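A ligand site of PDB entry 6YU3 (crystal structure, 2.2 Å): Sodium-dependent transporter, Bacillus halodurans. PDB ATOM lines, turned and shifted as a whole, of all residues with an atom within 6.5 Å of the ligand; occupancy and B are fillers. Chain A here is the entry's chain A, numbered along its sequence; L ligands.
OH of Tyr 110 lies within hydrogen-bond range of N of Leu 31 (2.9 Å). NE2 of Gln 229 is in hydrogen-bond range of O of Gly 32 (2.8 Å). The backbone carbonyl oxygen (O) of Ala 28 sits close to the side-chain amide oxygen (OD1) of Asn 33 (3.3 Å). The backbone NH of Gly 30 lies within hydrogen-bond range of the side-chain amide oxygen of Asn 33 (2.9 Å). OG of Ser 329 sits at hydrogen-bond distance from OG of Ser 27, at 2.8 Å. O of Ser 27 is in hydrogen-bond range of OG of Ser 326 (3.1 Å). The side-chain hydroxyl of Ser 329 is in hydrogen-bond range of the backbone carbonyl oxygen of Ser 326 (2.8 Å). ND2 of Asn 33 sits at hydrogen-bond distance from OD1 of Asp 265, 2.8 Å away.
The side-chain hydroxyl (OH) of Tyr 110 sits at hydrogen-bond distance from an oxygen (O1) of the ligand (2.8 Å). O1 of the ligand is in hydrogen-bond range of N of Gly 32 (2.8 Å). The side-chain hydroxyl (OG) of Ser 235 sits at hydrogen-bond distance from a nitrogen (N1) of the ligand, 2.9 Å away. The backbone carbonyl oxygen of Phe 232 sits at hydrogen-bond distance from a nitrogen (N1) of the ligand, 2.9 Å away. The backbone NH (N) of Leu 31 sits at hydrogen-bond distance from an oxygen (O1) of the ligand (2.9 Å). N1 of the ligand is in hydrogen-bond range of O of Ala 28, 3.1 Å away. The backbone carbonyl oxygen (O) of Thr 233 sits at hydrogen-bond distance from a nitrogen (N1) of the ligand (3.2 Å). The backbone carbonyl oxygen of Ser 27 is in hydrogen-bond range of a nitrogen (N1) of the ligand, 3.2 Å away.
Residues that only touch the ligand: Gly 30, Ser 329, Leu 330, Asn 33, Met 238, Ala 240 and Ser 326. Hydrophobic or aromatic side chains within 4 Å of the ligand: Tyr 110, Phe 232, Met 238, Ala 240 and Leu 330. 15 residues have an atom within 4 Å of the ligand: Ser 27, Ala 28, Gly 30, Leu 31, Gly 32, Asn 33, Tyr 110, Phe 232, Thr 233, Ser 235, Met 238, Ala 240, Ser 326, Ser 329 and Leu 330.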
ATOM      1  N   SER A  27       4.258   6.364   4.007  1.00  0.00           N
ATOM      2  CA  SER A  27       5.032   7.456   4.567  1.00  0.00           C
ATOM      3  C   SER A  27       4.476   7.906   5.910  1.00  0.00           C
ATOM      4  O   SER A  27       5.237   8.223   6.832  1.00  0.00           O
ATOM      5  CB  SER A  27       5.062   8.634   3.587  1.00  0.00           C
ATOM      6  OG  SER A  27       5.595   9.797   4.207  1.00  0.00           O
ATOM      7  N   ALA A  28       3.149   7.945   6.044  1.00  0.00           N
ATOM      8  CA  ALA A  28       2.535   8.434   7.281  1.00  0.00           C
ATOM      9  C   ALA A  28       2.719   7.438   8.420  1.00  0.00           C
ATOM     10  O   ALA A  28       3.236   7.792   9.486  1.00  0.00           O
ATOM     11  CB  ALA A  28       1.052   8.718   7.055  1.00  0.00           C
ATOM     12  N   VAL A  29       2.305   6.189   8.215  1.00  0.00           N
ATOM     13  CA  VAL A  29       2.325   5.186   9.277  1.00  0.00           C
ATOM     14  C   VAL A  29       3.764   4.753   9.509  1.00  0.00           C
ATOM     15  O   VAL A  29       4.379   4.126   8.647  1.00  0.00           O
ATOM     16  CB  VAL A  29       1.426   3.988   8.944  1.00  0.00           C
ATOM     17  CG1 VAL A  29       1.442   2.973  10.079  1.00  0.00           C
ATOM     18  CG2 VAL A  29       0.008   4.451   8.646  1.00  0.00           C
ATOM     19  N   GLY A  30       4.314   5.068  10.674  1.00  0.00           N
ATOM     20  CA  GLY A  30       5.675   4.701  11.004  1.00  0.00           C
ATOM     21  C   GLY A  30       5.928   4.837  12.487  1.00  0.00           C
ATOM     22  O   GLY A  30       5.041   4.595  13.319  1.00  0.00           O
ATOM     23  N   LEU A  31       7.153   5.228  12.832  1.00  0.00           N
ATOM     24  CA  LEU A  31       7.552   5.351  14.235  1.00  0.00           C
ATOM     25  C   LEU A  31       6.789   6.445  14.963  1.00  0.00           C
ATOM     26  O   LEU A  31       6.711   6.404  16.192  1.00  0.00           O
ATOM     27  CB  LEU A  31       9.062   5.622  14.335  1.00  0.00           C
ATOM     28  CG  LEU A  31      10.004   4.531  13.825  1.00  0.00           C
ATOM     29  CD1 LEU A  31      11.457   4.984  13.920  1.00  0.00           C
ATOM     30  CD2 LEU A  31       9.794   3.229  14.597  1.00  0.00           C
ATOM     31  N   GLY A  32       6.235   7.418  14.242  1.00  0.00           N
ATOM     32  CA  GLY A  32       5.481   8.483  14.879  1.00  0.00           C
ATOM     33  C   GLY A  32       4.168   8.032  15.473  1.00  0.00           C
ATOM     34  O   GLY A  32       3.667   8.676  16.408  1.00  0.00           O
ATOM     35  N   ASN A  33       3.587   6.948  14.965  1.00  0.00           N
ATOM     36  CA  ASN A  33       2.305   6.466  15.465  1.00  0.00           C
ATOM     37  C   ASN A  33       2.448   5.682  16.767  1.00  0.00           C
ATOM     38  O   ASN A  33       1.542   5.714  17.602  1.00  0.00           O
ATOM     39  CB  ASN A  33       1.626   5.573  14.421  1.00  0.00           C
ATOM     40  CG  ASN A  33       1.439   6.273  13.101  1.00  0.00           C
ATOM     41  OD1 ASN A  33       2.392   6.502  12.362  1.00  0.00           O
ATOM     42  ND2 ASN A  33       0.190   6.613  12.777  1.00  0.00           N
ATOM     43  N   ILE A 106      15.199  15.383  10.471  1.00  0.00           N
ATOM     44  CA  ILE A 106      14.296  14.345  10.957  1.00  0.00           C
ATOM     45  C   ILE A 106      14.876  12.969  10.701  1.00  0.00           C
ATOM     46  O   ILE A 106      14.914  12.114  11.598  1.00  0.00           O
ATOM     47  CB  ILE A 106      12.890  14.505  10.355  1.00  0.00           C
ATOM     48  CG1 ILE A 106      12.240  15.788  10.871  1.00  0.00           C
ATOM     49  CG2 ILE A 106      12.023  13.296  10.687  1.00  0.00           C
ATOM     50  CD1 ILE A 106      10.760  15.908  10.576  1.00  0.00           C
ATOM     51  N   TYR A 110      15.662   9.915  13.079  1.00  0.00           N
ATOM     52  CA  TYR A 110      14.715   8.839  12.764  1.00  0.00           C
ATOM     53  C   TYR A 110      15.446   7.518  12.564  1.00  0.00           C
ATOM     54  O   TYR A 110      14.958   6.463  12.983  1.00  0.00           O
ATOM     55  CB  TYR A 110      13.903   9.204  11.527  1.00  0.00           C
ATOM     56  CG  TYR A 110      12.595   8.442  11.372  1.00  0.00           C
ATOM     57  CD1 TYR A 110      11.412   8.961  11.877  1.00  0.00           C
ATOM     58  CD2 TYR A 110      12.555   7.219  10.717  1.00  0.00           C
ATOM     59  CE1 TYR A 110      10.218   8.270  11.732  1.00  0.00           C
ATOM     60  CE2 TYR A 110      11.365   6.519  10.572  1.00  0.00           C
ATOM     61  CZ  TYR A 110      10.198   7.056  11.083  1.00  0.00           C
ATOM     62  OH  TYR A 110       9.013   6.369  10.937  1.00  0.00           O
ATOM     63  N   GLN A 229       3.237  16.827  16.831  1.00  0.00           N
ATOM     64  CA  GLN A 229       2.917  15.423  16.594  1.00  0.00           C
ATOM     65  C   GLN A 229       1.988  15.260  15.401  1.00  0.00           C
ATOM     66  O   GLN A 229       2.117  14.316  14.630  1.00  0.00           O
ATOM     67  CB  GLN A 229       2.309  14.805  17.849  1.00  0.00           C
ATOM     68  CG  GLN A 229       1.898  13.341  17.699  1.00  0.00           C
ATOM     69  CD  GLN A 229       3.077  12.409  17.488  1.00  0.00           C
ATOM     70  OE1 GLN A 229       4.203  12.714  17.873  1.00  0.00           O
ATOM     71  NE2 GLN A 229       2.812  11.264  16.869  1.00  0.00           N
ATOM     72  N   PHE A 231       1.745  17.270  12.677  1.00  0.00           N
ATOM     73  CA  PHE A 231       2.547  17.429  11.468  1.00  0.00           C
ATOM     74  C   PHE A 231       3.475  16.236  11.261  1.00  0.00           C
ATOM     75  O   PHE A 231       3.593  15.719  10.148  1.00  0.00           O
ATOM     76  CB  PHE A 231       3.358  18.727  11.543  1.00  0.00           C
ATOM     77  CG  PHE A 231       2.555  19.953  10.961  1.00  0.00           C
ATOM     78  CD1 PHE A 231       1.857  20.794  11.819  1.00  0.00           C
ATOM     79  CD2 PHE A 231       2.571  20.206   9.583  1.00  0.00           C
ATOM     80  CE1 PHE A 231       1.159  21.881  11.313  1.00  0.00           C
ATOM     81  CE2 PHE A 231       1.877  21.284   9.077  1.00  0.00           C
ATOM     82  CZ  PHE A 231       1.158  22.127   9.938  1.00  0.00           C
ATOM     83  N   PHE A 232       4.129  15.790  12.335  1.00  0.00           N
ATOM     84  CA  PHE A 232       5.114  14.711  12.233  1.00  0.00           C
ATOM     85  C   PHE A 232       4.468  13.424  11.739  1.00  0.00           C
ATOM     86  O   PHE A 232       4.951  12.794  10.795  1.00  0.00           O
ATOM     87  CB  PHE A 232       5.781  14.501  13.591  1.00  0.00           C
ATOM     88  CG  PHE A 232       6.949  13.447  13.522  1.00  0.00           C
ATOM     89  CD1 PHE A 232       6.695  12.098  13.737  1.00  0.00           C
ATOM     90  CD2 PHE A 232       8.261  13.880  13.264  1.00  0.00           C
ATOM     91  CE1 PHE A 232       7.724  11.170  13.688  1.00  0.00           C
ATOM     92  CE2 PHE A 232       9.291  12.951  13.216  1.00  0.00           C
ATOM     93  CZ  PHE A 232       9.017  11.594  13.424  1.00  0.00           C
ATOM     94  N   THR A 233       3.363  13.020  12.370  1.00  0.00           N
ATOM     95  CA  THR A 233       2.730  11.741  12.036  1.00  0.00           C
ATOM     96  C   THR A 233       2.105  11.739  10.647  1.00  0.00           C
ATOM     97  O   THR A 233       1.952  10.654  10.058  1.00  0.00           O
ATOM     98  CB  THR A 233       1.657  11.410  13.103  1.00  0.00           C
ATOM     99  OG1 THR A 233       1.279  10.036  12.983  1.00  0.00           O
ATOM    100  CG2 THR A 233       0.424  12.292  12.941  1.00  0.00           C
ATOM    101  N   LEU A 234       1.785  12.902  10.091  1.00  0.00           N
ATOM    102  CA  LEU A 234       1.188  12.989   8.762  1.00  0.00           C
ATOM    103  C   LEU A 234       2.217  13.202   7.659  1.00  0.00           C
ATOM    104  O   LEU A 234       1.810  13.374   6.500  1.00  0.00           O
ATOM    105  CB  LEU A 234       0.156  14.111   8.706  1.00  0.00           C
ATOM    106  CG  LEU A 234      -1.123  13.906   9.530  1.00  0.00           C
ATOM    107  CD1 LEU A 234      -2.047  15.096   9.372  1.00  0.00           C
ATOM    108  CD2 LEU A 234      -1.823  12.619   9.105  1.00  0.00           C
ATOM    109  N   SER A 235       3.508  13.197   7.973  1.00  0.00           N
ATOM    110  CA  SER A 235       4.559  13.487   7.003  1.00  0.00           C
ATOM    111  C   SER A 235       4.287  14.821   6.317  1.00  0.00           C
ATOM    112  O   SER A 235       4.367  14.962   5.091  1.00  0.00           O
ATOM    113  CB  SER A 235       4.678  12.361   5.974  1.00  0.00           C
ATOM    114  OG  SER A 235       4.749  11.092   6.612  1.00  0.00           O
ATOM    115  N   LEU A 236       3.949  15.828   7.122  1.00  0.00           N
ATOM    116  CA  LEU A 236       3.350  17.056   6.643  1.00  0.00           C
ATOM    117  C   LEU A 236       4.243  18.251   6.936  1.00  0.00           C
ATOM    118  O   LEU A 236       4.947  18.305   7.956  1.00  0.00           O
ATOM    119  CB  LEU A 236       1.973  17.265   7.289  1.00  0.00           C
ATOM    120  CG  LEU A 236       1.068  18.327   6.672  1.00  0.00           C
ATOM    121  CD1 LEU A 236       0.911  18.068   5.184  1.00  0.00           C
ATOM    122  CD2 LEU A 236      -0.276  18.354   7.377  1.00  0.00           C
ATOM    123  N   MET A 238       6.810  19.468   5.046  1.00  0.00           N
ATOM    124  CA  MET A 238       8.173  19.430   4.552  1.00  0.00           C
ATOM    125  C   MET A 238       8.260  19.091   3.065  1.00  0.00           C
ATOM    126  O   MET A 238       9.366  18.899   2.548  1.00  0.00           O
ATOM    127  CB  MET A 238       9.020  18.443   5.343  1.00  0.00           C
ATOM    128  CG  MET A 238       8.663  16.990   5.084  1.00  0.00           C
ATOM    129  SD  MET A 238      10.063  15.898   5.370  1.00  0.00           S
ATOM    130  CE  MET A 238      10.466  16.330   7.053  1.00  0.00           C
ATOM    131  N   ALA A 240       7.238  16.305   1.771  1.00  0.00           N
ATOM    132  CA  ALA A 240       7.288  14.854   1.576  1.00  0.00           C
ATOM    133  C   ALA A 240       6.069  14.374   0.791  1.00  0.00           C
ATOM    134  O   ALA A 240       6.189  13.512  -0.085  1.00  0.00           O
ATOM    135  CB  ALA A 240       7.387  14.139   2.920  1.00  0.00           C
ATOM    136  N   ASP A 265      -3.804   6.880   9.649  1.00  0.00           N
ATOM    137  CA  ASP A 265      -2.716   7.229  10.563  1.00  0.00           C
ATOM    138  C   ASP A 265      -3.236   7.424  11.989  1.00  0.00           C
ATOM    139  O   ASP A 265      -2.563   7.039  12.955  1.00  0.00           O
ATOM    140  CB  ASP A 265      -2.022   8.493  10.069  1.00  0.00           C
ATOM    141  CG  ASP A 265      -0.777   8.821  10.882  1.00  0.00           C
ATOM    142  OD1 ASP A 265       0.293   8.255  10.568  1.00  0.00           O
ATOM    143  OD2 ASP A 265      -0.882   9.625  11.830  1.00  0.00           O
ATOM    144  N   ALA A 322       7.446  -0.616   8.738  1.00  0.00           N
ATOM    145  CA  ALA A 322       6.785   0.677   8.637  1.00  0.00           C
ATOM    146  C   ALA A 322       7.789   1.820   8.806  1.00  0.00           C
ATOM    147  O   ALA A 322       7.671   2.862   8.161  1.00  0.00           O
ATOM    148  CB  ALA A 322       5.667   0.794   9.667  1.00  0.00           C
ATOM    149  N   ALA A 323       8.779   1.636   9.682  1.00  0.00           N
ATOM    150  CA  ALA A 323       9.820   2.653   9.815  1.00  0.00           C
ATOM    151  C   ALA A 323      10.629   2.792   8.526  1.00  0.00           C
ATOM    152  O   ALA A 323      11.052   3.896   8.173  1.00  0.00           O
ATOM    153  CB  ALA A 323      10.742   2.312  10.985  1.00  0.00           C
ATOM    154  N   SER A 326       8.736   4.854   5.952  1.00  0.00           N
ATOM    155  CA  SER A 326       8.664   6.254   6.336  1.00  0.00           C
ATOM    156  C   SER A 326      10.005   6.950   6.136  1.00  0.00           C
ATOM    157  O   SER A 326      10.049   8.108   5.692  1.00  0.00           O
ATOM    158  CB  SER A 326       8.211   6.380   7.789  1.00  0.00           C
ATOM    159  OG  SER A 326       6.878   5.905   7.951  1.00  0.00           O
ATOM    160  N   ALA A 327      11.109   6.275   6.444  1.00  0.00           N
ATOM    161  CA  ALA A 327      12.427   6.864   6.225  1.00  0.00           C
ATOM    162  C   ALA A 327      12.739   7.003   4.742  1.00  0.00           C
ATOM    163  O   ALA A 327      13.536   7.866   4.354  1.00  0.00           O
ATOM    164  CB  ALA A 327      13.504   6.018   6.913  1.00  0.00           C
ATOM    165  N   SER A 329      10.505   7.952   2.398  1.00  0.00           N
ATOM    166  CA  SER A 329       9.902   9.223   2.007  1.00  0.00           C
ATOM    167  C   SER A 329      10.675  10.402   2.582  1.00  0.00           C
ATOM    168  O   SER A 329      10.691  11.480   1.975  1.00  0.00           O
ATOM    169  CB  SER A 329       8.451   9.288   2.441  1.00  0.00           C
ATOM    170  OG  SER A 329       8.338   9.397   3.847  1.00  0.00           O
ATOM    171  N   LEU A 330      11.291  10.234   3.752  1.00  0.00           N
ATOM    172  CA  LEU A 330      12.121  11.295   4.307  1.00  0.00           C
ATOM    173  C   LEU A 330      13.335  11.548   3.418  1.00  0.00           C
ATOM    174  O   LEU A 330      13.658  12.697   3.107  1.00  0.00           O
ATOM    175  CB  LEU A 330      12.569  10.927   5.728  1.00  0.00           C
ATOM    176  CG  LEU A 330      11.581  11.265   6.846  1.00  0.00           C
ATOM    177  CD1 LEU A 330      11.919  10.499   8.109  1.00  0.00           C
ATOM    178  CD2 LEU A 330      11.588  12.763   7.102  1.00  0.00           C
ATOM    179  N   VAL A 333      12.872  13.431  -0.257  1.00  0.00           N
ATOM    180  CA  VAL A 333      12.720  14.878  -0.411  1.00  0.00           C
ATOM    181  C   VAL A 333      14.053  15.525  -0.779  1.00  0.00           C
ATOM    182  O   VAL A 333      14.100  16.275  -1.771  1.00  0.00           O
ATOM    183  CB  VAL A 333      12.115  15.513   0.854  1.00  0.00           C
ATOM    184  CG1 VAL A 333      11.957  17.011   0.666  1.00  0.00           C
ATOM    185  CG2 VAL A 333      10.783  14.866   1.170  1.00  0.00           C
ATOM    186  N   LEU A 395       8.341  22.172  10.486  1.00  0.00           N
ATOM    187  CA  LEU A 395       7.115  21.539   9.987  1.00  0.00           C
ATOM    188  C   LEU A 395       5.889  22.428  10.137  1.00  0.00           C
ATOM    189  O   LEU A 395       5.162  22.593   9.144  1.00  0.00           O
ATOM    190  CB  LEU A 395       6.914  20.175  10.661  1.00  0.00           C
ATOM    191  CG  LEU A 395       7.938  19.078  10.352  1.00  0.00           C
ATOM    192  CD1 LEU A 395       7.423  17.739  10.866  1.00  0.00           C
ATOM    193  CD2 LEU A 395       8.256  19.002   8.874  1.00  0.00           C
HETATM  194  N1  LIG L   1       5.089  10.235   9.380  1.00  0.00           N
HETATM  195  C1  LIG L   1       6.249   9.543   9.843  1.00  0.00           C
HETATM  196  C2  LIG L   1       5.923   8.763  11.120  1.00  0.00           C
HETATM  197  O1  LIG L   1       6.682   7.809  11.487  1.00  0.00           O
HETATM  198  C3  LIG L   1       7.410  10.536  10.103  1.00  0.00           C
HETATM  199  C4  LIG L   1       7.685  11.403   8.816  1.00  0.00           C
HETATM  200  C5  LIG L   1       7.839  10.781   7.584  1.00  0.00           C
HETATM  201  C6  LIG L   1       7.777  12.795   8.915  1.00  0.00           C
HETATM  202  C7  LIG L   1       8.088  11.540   6.451  1.00  0.00           C
HETATM  203  C8  LIG L   1       8.026  13.554   7.782  1.00  0.00           C
HETATM  204  C9  LIG L   1       8.183  12.921   6.540  1.00  0.00           C
HETATM  205  O2  LIG L   1       4.912   9.064  11.819  1.00  0.00           O
